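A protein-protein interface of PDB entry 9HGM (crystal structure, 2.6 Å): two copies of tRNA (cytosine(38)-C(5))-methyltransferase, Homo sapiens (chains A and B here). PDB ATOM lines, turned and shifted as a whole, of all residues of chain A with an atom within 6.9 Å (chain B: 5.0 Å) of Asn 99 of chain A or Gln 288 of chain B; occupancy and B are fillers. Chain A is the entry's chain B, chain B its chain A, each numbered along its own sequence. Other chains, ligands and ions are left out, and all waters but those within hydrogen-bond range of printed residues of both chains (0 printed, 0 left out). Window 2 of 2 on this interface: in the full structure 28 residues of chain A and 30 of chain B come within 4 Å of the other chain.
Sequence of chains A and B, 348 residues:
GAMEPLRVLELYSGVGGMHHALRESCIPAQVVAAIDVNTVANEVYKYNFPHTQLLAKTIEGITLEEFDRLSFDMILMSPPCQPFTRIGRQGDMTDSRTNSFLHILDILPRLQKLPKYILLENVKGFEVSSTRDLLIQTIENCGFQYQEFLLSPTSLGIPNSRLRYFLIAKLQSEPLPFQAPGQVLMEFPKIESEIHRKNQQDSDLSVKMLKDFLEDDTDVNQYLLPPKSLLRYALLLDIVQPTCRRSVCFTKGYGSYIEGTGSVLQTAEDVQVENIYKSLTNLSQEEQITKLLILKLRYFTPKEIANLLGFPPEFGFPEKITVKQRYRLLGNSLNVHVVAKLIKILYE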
ATOM      1  N   TYR A  12      -5.142  -9.864  19.207  1.00  0.00           N
ATOM      2  CA  TYR A  12      -6.350  -9.513  19.948  1.00  0.00           C
ATOM      3  C   TYR A  12      -6.942 -10.764  20.606  1.00  0.00           C
ATOM      4  O   TYR A  12      -8.069 -11.176  20.331  1.00  0.00           O
ATOM      5  CB  TYR A  12      -7.363  -8.830  19.036  1.00  0.00           C
ATOM      6  CG  TYR A  12      -6.958  -7.456  18.552  1.00  0.00           C
ATOM      7  CD1 TYR A  12      -6.277  -6.575  19.382  1.00  0.00           C
ATOM      8  CD2 TYR A  12      -7.255  -7.039  17.259  1.00  0.00           C
ATOM      9  CE1 TYR A  12      -5.902  -5.312  18.935  1.00  0.00           C
ATOM     10  CE2 TYR A  12      -6.885  -5.778  16.802  1.00  0.00           C
ATOM     11  CZ  TYR A  12      -6.212  -4.924  17.643  1.00  0.00           C
ATOM     12  OH  TYR A  12      -5.845  -3.676  17.196  1.00  0.00           O
ATOM     13  N   ILE A  59      -0.376  -4.075  19.162  1.00  0.00           N
ATOM     14  CA  ILE A  59       0.292  -4.670  18.009  1.00  0.00           C
ATOM     15  C   ILE A  59       1.272  -3.693  17.378  1.00  0.00           C
ATOM     16  O   ILE A  59       2.322  -4.101  16.871  1.00  0.00           O
ATOM     17  CB  ILE A  59      -0.746  -5.160  16.989  1.00  0.00           C
ATOM     18  CG1 ILE A  59      -1.503  -6.359  17.553  1.00  0.00           C
ATOM     19  CG2 ILE A  59      -0.067  -5.515  15.680  1.00  0.00           C
ATOM     20  CD1 ILE A  59      -2.603  -6.843  16.663  1.00  0.00           C
ATOM     21  N   GLU A  60       0.956  -2.393  17.395  1.00  0.00           N
ATOM     22  CA  GLU A  60       1.853  -1.414  16.800  1.00  0.00           C
ATOM     23  C   GLU A  60       3.134  -1.241  17.603  1.00  0.00           C
ATOM     24  O   GLU A  60       4.143  -0.792  17.047  1.00  0.00           O
ATOM     25  CB  GLU A  60       1.144  -0.063  16.647  1.00  0.00           C
ATOM     26  CG  GLU A  60       0.547   0.476  17.938  1.00  0.00           C
ATOM     27  CD  GLU A  60       0.342   1.978  17.908  1.00  0.00           C
ATOM     28  OE1 GLU A  60       0.997   2.656  17.084  1.00  0.00           O
ATOM     29  OE2 GLU A  60      -0.474   2.485  18.705  1.00  0.00           O
ATOM     30  N   ASP A  95      -8.062   4.386  20.665  1.00  0.00           N
ATOM     31  CA  ASP A  95      -8.133   3.379  19.607  1.00  0.00           C
ATOM     32  C   ASP A  95      -6.808   3.356  18.862  1.00  0.00           C
ATOM     33  O   ASP A  95      -6.515   4.233  18.047  1.00  0.00           O
ATOM     34  CB  ASP A  95      -9.291   3.656  18.661  1.00  0.00           C
ATOM     35  CG  ASP A  95     -10.349   2.581  18.720  1.00  0.00           C
ATOM     36  OD1 ASP A  95     -10.037   1.469  19.195  1.00  0.00           O
ATOM     37  OD2 ASP A  95     -11.495   2.849  18.291  1.00  0.00           O
ATOM     38  N   SER A  96      -6.001   2.339  19.147  1.00  0.00           N
ATOM     39  CA  SER A  96      -4.799   2.081  18.386  1.00  0.00           C
ATOM     40  C   SER A  96      -5.062   1.166  17.199  1.00  0.00           C
ATOM     41  O   SER A  96      -4.114   0.631  16.616  1.00  0.00           O
ATOM     42  CB  SER A  96      -3.735   1.468  19.294  1.00  0.00           C
ATOM     43  OG  SER A  96      -4.251   0.311  19.932  1.00  0.00           O
ATOM     44  N   ARG A  97      -6.328   0.982  16.824  1.00  0.00           N
ATOM     45  CA  ARG A  97      -6.662  -0.031  15.831  1.00  0.00           C
ATOM     46  C   ARG A  97      -6.079   0.317  14.466  1.00  0.00           C
ATOM     47  O   ARG A  97      -5.459  -0.529  13.817  1.00  0.00           O
ATOM     48  CB  ARG A  97      -8.176  -0.215  15.757  1.00  0.00           C
ATOM     49  CG  ARG A  97      -8.764  -0.867  16.998  1.00  0.00           C
ATOM     50  CD  ARG A  97     -10.234  -1.225  16.832  1.00  0.00           C
ATOM     51  NE  ARG A  97     -11.126  -0.091  17.060  1.00  0.00           N
ATOM     52  CZ  ARG A  97     -12.446  -0.182  17.119  1.00  0.00           C
ATOM     53  NH1 ARG A  97     -13.065  -1.349  16.992  1.00  0.00           N
ATOM     54  NH2 ARG A  97     -13.168   0.920  17.316  1.00  0.00           N
ATOM     55  N   THR A  98      -6.269   1.552  14.011  1.00  0.00           N
ATOM     56  CA  THR A  98      -5.758   1.935  12.696  1.00  0.00           C
ATOM     57  C   THR A  98      -4.258   1.681  12.607  1.00  0.00           C
ATOM     58  O   THR A  98      -3.777   1.020  11.676  1.00  0.00           O
ATOM     59  CB  THR A  98      -6.083   3.399  12.405  1.00  0.00           C
ATOM     60  OG1 THR A  98      -7.503   3.582  12.449  1.00  0.00           O
ATOM     61  CG2 THR A  98      -5.571   3.791  11.028  1.00  0.00           C
ATOM     62  N   ASN A  99      -3.501   2.176  13.592  1.00  0.00           N
ATOM     63  CA  ASN A  99      -2.056   1.971  13.601  1.00  0.00           C
ATOM     64  C   ASN A  99      -1.695   0.500  13.782  1.00  0.00           C
ATOM     65  O   ASN A  99      -0.756   0.006  13.146  1.00  0.00           O
ATOM     66  CB  ASN A  99      -1.411   2.821  14.695  1.00  0.00           C
ATOM     67  CG  ASN A  99      -1.210   4.245  14.264  1.00  0.00           C
ATOM     68  OD1 ASN A  99      -1.311   4.564  13.074  1.00  0.00           O
ATOM     69  ND2 ASN A  99      -0.914   5.118  15.220  1.00  0.00           N
ATOM     70  N   SER A 100      -2.414  -0.218  14.647  1.00  0.00           N
ATOM     71  CA  SER A 100      -2.131  -1.638  14.825  1.00  0.00           C
ATOM     72  C   SER A 100      -2.389  -2.416  13.539  1.00  0.00           C
ATOM     73  O   SER A 100      -1.598  -3.288  13.162  1.00  0.00           O
ATOM     74  CB  SER A 100      -2.962  -2.208  15.974  1.00  0.00           C
ATOM     75  OG  SER A 100      -2.596  -1.616  17.208  1.00  0.00           O
ATOM     76  N   PHE A 101      -3.494  -2.122  12.852  1.00  0.00           N
ATOM     77  CA  PHE A 101      -3.793  -2.820  11.608  1.00  0.00           C
ATOM     78  C   PHE A 101      -2.775  -2.483  10.532  1.00  0.00           C
ATOM     79  O   PHE A 101      -2.368  -3.360   9.759  1.00  0.00           O
ATOM     80  CB  PHE A 101      -5.201  -2.478  11.128  1.00  0.00           C
ATOM     81  CG  PHE A 101      -5.553  -3.101   9.811  1.00  0.00           C
ATOM     82  CD1 PHE A 101      -5.852  -4.444   9.724  1.00  0.00           C
ATOM     83  CD2 PHE A 101      -5.590  -2.336   8.653  1.00  0.00           C
ATOM     84  CE1 PHE A 101      -6.184  -5.025   8.517  1.00  0.00           C
ATOM     85  CE2 PHE A 101      -5.921  -2.909   7.436  1.00  0.00           C
ATOM     86  CZ  PHE A 101      -6.220  -4.256   7.368  1.00  0.00           C
ATOM     87  N   LEU A 102      -2.358  -1.219  10.453  1.00  0.00           N
ATOM     88  CA  LEU A 102      -1.333  -0.855   9.482  1.00  0.00           C
ATOM     89  C   LEU A 102      -0.001  -1.544   9.790  1.00  0.00           C
ATOM     90  O   LEU A 102       0.702  -1.987   8.876  1.00  0.00           O
ATOM     91  CB  LEU A 102      -1.157   0.659   9.443  1.00  0.00           C
ATOM     92  CG  LEU A 102      -2.292   1.410   8.761  1.00  0.00           C
ATOM     93  CD1 LEU A 102      -1.955   2.877   8.680  1.00  0.00           C
ATOM     94  CD2 LEU A 102      -2.547   0.830   7.380  1.00  0.00           C
ATOM     95  N   HIS A 103       0.362  -1.643  11.075  1.00  0.00           N
ATOM     96  CA  HIS A 103       1.616  -2.295  11.426  1.00  0.00           C
ATOM     97  C   HIS A 103       1.602  -3.759  11.013  1.00  0.00           C
ATOM     98  O   HIS A 103       2.630  -4.310  10.590  1.00  0.00           O
ATOM     99  CB  HIS A 103       1.887  -2.164  12.926  1.00  0.00           C
ATOM    100  CG  HIS A 103       3.298  -2.486  13.315  1.00  0.00           C
ATOM    101  ND1 HIS A 103       4.388  -2.026  12.605  1.00  0.00           N
ATOM    102  CD2 HIS A 103       3.797  -3.211  14.346  1.00  0.00           C
ATOM    103  CE1 HIS A 103       5.497  -2.458  13.179  1.00  0.00           C
ATOM    104  NE2 HIS A 103       5.167  -3.179  14.237  1.00  0.00           N
ATOM    105  N   ILE A 104       0.449  -4.407  11.129  1.00  0.00           N
ATOM    106  CA  ILE A 104       0.338  -5.797  10.688  1.00  0.00           C
ATOM    107  C   ILE A 104       0.589  -5.889   9.192  1.00  0.00           C
ATOM    108  O   ILE A 104       1.365  -6.733   8.723  1.00  0.00           O
ATOM    109  CB  ILE A 104      -1.034  -6.373  11.070  1.00  0.00           C
ATOM    110  CG1 ILE A 104      -1.165  -6.468  12.594  1.00  0.00           C
ATOM    111  CG2 ILE A 104      -1.216  -7.729  10.435  1.00  0.00           C
ATOM    112  CD1 ILE A 104      -2.587  -6.689  13.070  1.00  0.00           C
ATOM    113  N   LEU B 231     -10.256  10.245  12.623  1.00  0.00           N
ATOM    114  CA  LEU B 231      -8.991   9.628  13.010  1.00  0.00           C
ATOM    115  C   LEU B 231      -9.192   8.315  13.761  1.00  0.00           C
ATOM    116  O   LEU B 231      -8.410   7.377  13.580  1.00  0.00           O
ATOM    117  CB  LEU B 231      -8.182  10.590  13.877  1.00  0.00           C
ATOM    118  CG  LEU B 231      -6.874  10.062  14.472  1.00  0.00           C
ATOM    119  CD1 LEU B 231      -5.818   9.914  13.387  1.00  0.00           C
ATOM    120  CD2 LEU B 231      -6.382  10.970  15.592  1.00  0.00           C
ATOM    121  N   LEU B 280      -1.197   6.566   5.682  1.00  0.00           N
ATOM    122  CA  LEU B 280      -1.231   6.809   7.118  1.00  0.00           C
ATOM    123  C   LEU B 280      -0.119   6.074   7.848  1.00  0.00           C
ATOM    124  O   LEU B 280       0.091   6.326   9.040  1.00  0.00           O
ATOM    125  CB  LEU B 280      -2.588   6.392   7.694  1.00  0.00           C
ATOM    126  CG  LEU B 280      -3.879   7.057   7.191  1.00  0.00           C
ATOM    127  CD1 LEU B 280      -5.102   6.330   7.740  1.00  0.00           C
ATOM    128  CD2 LEU B 280      -3.931   8.534   7.564  1.00  0.00           C
ATOM    129  N   THR B 281       0.601   5.192   7.161  1.00  0.00           N
ATOM    130  CA  THR B 281       1.540   4.295   7.823  1.00  0.00           C
ATOM    131  C   THR B 281       2.725   5.070   8.383  1.00  0.00           C
ATOM    132  O   THR B 281       3.369   5.845   7.673  1.00  0.00           O
ATOM    133  CB  THR B 281       2.023   3.224   6.848  1.00  0.00           C
ATOM    134  OG1 THR B 281       0.893   2.508   6.342  1.00  0.00           O
ATOM    135  CG2 THR B 281       2.951   2.245   7.552  1.00  0.00           C
ATOM    136  N   LEU B 283       2.885   7.563  10.063  1.00  0.00           N
ATOM    137  CA  LEU B 283       2.663   8.980  10.275  1.00  0.00           C
ATOM    138  C   LEU B 283       2.102   9.229  11.673  1.00  0.00           C
ATOM    139  O   LEU B 283       1.546   8.335  12.321  1.00  0.00           O
ATOM    140  CB  LEU B 283       1.713   9.537   9.218  1.00  0.00           C
ATOM    141  CG  LEU B 283       2.256   9.544   7.794  1.00  0.00           C
ATOM    142  CD1 LEU B 283       1.377  10.430   6.919  1.00  0.00           C
ATOM    143  CD2 LEU B 283       3.707  10.012   7.774  1.00  0.00           C
ATOM    144  N   SER B 284       2.263  10.470  12.140  1.00  0.00           N
ATOM    145  CA  SER B 284       1.775  10.843  13.458  1.00  0.00           C
ATOM    146  C   SER B 284       0.274  11.105  13.414  1.00  0.00           C
ATOM    147  O   SER B 284      -0.337  11.226  12.347  1.00  0.00           O
ATOM    148  CB  SER B 284       2.495  12.083  13.966  1.00  0.00           C
ATOM    149  OG  SER B 284       1.947  13.259  13.386  1.00  0.00           O
ATOM    150  N   GLN B 285      -0.321  11.203  14.604  1.00  0.00           N
ATOM    151  CA  GLN B 285      -1.751  11.484  14.718  1.00  0.00           C
ATOM    152  C   GLN B 285      -2.138  12.692  13.872  1.00  0.00           C
ATOM    153  O   GLN B 285      -3.000  12.601  12.989  1.00  0.00           O
ATOM    154  CB  GLN B 285      -2.127  11.706  16.182  1.00  0.00           C
ATOM    155  CG  GLN B 285      -1.856  10.514  17.077  1.00  0.00           C
ATOM    156  CD  GLN B 285      -2.893   9.427  16.918  1.00  0.00           C
ATOM    157  OE1 GLN B 285      -4.085   9.663  17.121  1.00  0.00           O
ATOM    158  NE2 GLN B 285      -2.448   8.227  16.544  1.00  0.00           N
ATOM    159  N   GLU B 286      -1.505  13.839  14.124  1.00  0.00           N
ATOM    160  CA  GLU B 286      -1.862  15.050  13.394  1.00  0.00           C
ATOM    161  C   GLU B 286      -1.546  14.924  11.910  1.00  0.00           C
ATOM    162  O   GLU B 286      -2.276  15.467  11.073  1.00  0.00           O
ATOM    163  CB  GLU B 286      -1.143  16.263  13.991  1.00  0.00           C
ATOM    164  CG  GLU B 286      -1.435  16.516  15.465  1.00  0.00           C
ATOM    165  CD  GLU B 286      -0.622  15.624  16.388  1.00  0.00           C
ATOM    166  OE1 GLU B 286       0.423  15.095  15.944  1.00  0.00           O
ATOM    167  OE2 GLU B 286      -1.029  15.451  17.559  1.00  0.00           O
ATOM    168  N   GLU B 287      -0.471  14.220  11.561  1.00  0.00           N
ATOM    169  CA  GLU B 287      -0.152  14.029  10.149  1.00  0.00           C
ATOM    170  C   GLU B 287      -1.142  13.084   9.484  1.00  0.00           C
ATOM    171  O   GLU B 287      -1.483  13.259   8.309  1.00  0.00           O
ATOM    172  CB  GLU B 287       1.276  13.511  10.001  1.00  0.00           C
ATOM    173  CG  GLU B 287       2.322  14.487  10.491  1.00  0.00           C
ATOM    174  CD  GLU B 287       3.667  13.838  10.693  1.00  0.00           C
ATOM    175  OE1 GLU B 287       3.775  12.609  10.485  1.00  0.00           O
ATOM    176  OE2 GLU B 287       4.622  14.558  11.066  1.00  0.00           O
ATOM    177  N   GLN B 288      -1.618  12.074  10.216  1.00  0.00           N
ATOM    178  CA  GLN B 288      -2.662  11.202   9.680  1.00  0.00           C
ATOM    179  C   GLN B 288      -3.960  11.970   9.480  1.00  0.00           C
ATOM    180  O   GLN B 288      -4.604  11.860   8.426  1.00  0.00           O
ATOM    181  CB  GLN B 288      -2.879  10.006  10.613  1.00  0.00           C
ATOM    182  CG  GLN B 288      -1.749   8.992  10.582  1.00  0.00           C
ATOM    183  CD  GLN B 288      -1.891   7.919  11.637  1.00  0.00           C
ATOM    184  OE1 GLN B 288      -2.382   8.170  12.739  1.00  0.00           O
ATOM    185  NE2 GLN B 288      -1.463   6.707  11.305  1.00  0.00           N
ATOM    186  N   ILE B 289      -4.364  12.753  10.485  1.00  0.00           N
ATOM    187  CA  ILE B 289      -5.591  13.546  10.395  1.00  0.00           C
ATOM    188  C   ILE B 289      -5.582  14.399   9.140  1.00  0.00           C
ATOM    189  O   ILE B 289      -6.634  14.649   8.527  1.00  0.00           O
ATOM    190  CB  ILE B 289      -5.749  14.431  11.663  1.00  0.00           C
ATOM    191  CG1 ILE B 289      -6.039  13.581  12.911  1.00  0.00           C
ATOM    192  CG2 ILE B 289      -6.834  15.482  11.433  1.00  0.00           C
ATOM    193  CD1 ILE B 289      -6.429  14.397  14.143  1.00  0.00           C
ATOM    194  N   THR B 290      -4.406  14.860   8.729  1.00  0.00           N
ATOM    195  CA  THR B 290      -4.330  15.756   7.585  1.00  0.00           C
ATOM    196  C   THR B 290      -4.529  15.010   6.272  1.00  0.00           C
ATOM    197  O   THR B 290      -5.177  15.521   5.357  1.00  0.00           O
ATOM    198  CB  THR B 290      -2.995  16.486   7.599  1.00  0.00           C
ATOM    199  OG1 THR B 290      -2.947  17.322   8.762  1.00  0.00           O
ATOM    200  CG2 THR B 290      -2.856  17.334   6.357  1.00  0.00           C
ATOM    201  N   LYS B 291      -3.979  13.796   6.159  1.00  0.00           N
ATOM    202  CA  LYS B 291      -4.130  13.040   4.921  1.00  0.00           C
ATOM    203  C   LYS B 291      -5.563  12.565   4.726  1.00  0.00           C
ATOM    204  O   LYS B 291      -6.010  12.392   3.582  1.00  0.00           O
ATOM    205  CB  LYS B 291      -3.173  11.845   4.914  1.00  0.00           C
ATOM    206  CG  LYS B 291      -1.745  12.185   4.514  1.00  0.00           C
ATOM    207  CD  LYS B 291      -1.589  12.286   2.999  1.00  0.00           C
ATOM    208  CE  LYS B 291      -0.152  12.617   2.604  1.00  0.00           C
ATOM    209  NZ  LYS B 291       0.024  12.622   1.124  1.00  0.00           N
ATOM    210  N   LEU B 292      -6.295  12.348   5.820  1.00  0.00           N
ATOM    211  CA  LEU B 292      -7.653  11.823   5.708  1.00  0.00           C
ATOM    212  C   LEU B 292      -8.645  12.909   5.304  1.00  0.00           C
ATOM    213  O   LEU B 292      -9.599  12.634   4.562  1.00  0.00           O
ATOM    214  CB  LEU B 292      -8.082  11.178   7.033  1.00  0.00           C
ATOM    215  CG  LEU B 292      -7.404   9.857   7.408  1.00  0.00           C
ATOM    216  CD1 LEU B 292      -7.554   9.551   8.897  1.00  0.00           C
ATOM    217  CD2 LEU B 292      -7.974   8.719   6.576  1.00  0.00           C
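NE2 of Gln 288 of chain B is in hydrogen-bond range of OD1 of Asn 99 of chain A, at 2.8 Å.
The backbone carbonyl oxygen of Leu 280 of chain B lies within hydrogen-bond range of the side-chain amide nitrogen of Gln 288 of chain B.
Asn 99 of chain A touches Gln 285 of chain B (ND2 to NE2, 3.7 Å). CD1 of Leu 102 of chain A touches CB of Leu 280 of chain B, 3.7 Å away. CD1 of Leu 102 of chain A touches OG1 of Thr 281 of chain B (3.7 Å).
Gln 288 of chain B touches one residue of chain A. Of the printed residues of chain A, Leu 280 of chain B touches Leu 102. Of the printed residues of chain A, Thr 281 of chain B touches Leu 102 (3.7 Å). The nearest residue of chain B that does not touch Asn 99 of chain A is Leu 280 of chain B (4.6 Å). The nearest residue of chain A that does not touch Gln 288 of chain B is Leu 102 of chain A (4.7 Å). The nearest printed residue of chain A that does not touch Gln 285 of chain B is Asp 95 of chain A (5.9 Å).
Of the 13 printed residues of chain B, 4 touch a printed residue of chain A. Hydrophobic or aromatic side chains of chain B within 4 Å of the printed part of chain A: Leu 280. Among the printed residues, 4 pairs touch across the chains.
No position is printed for both chains. Of the 4 pairs that touch across the chains among the printed residues, none has its exchanged pair printed and touching as well.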
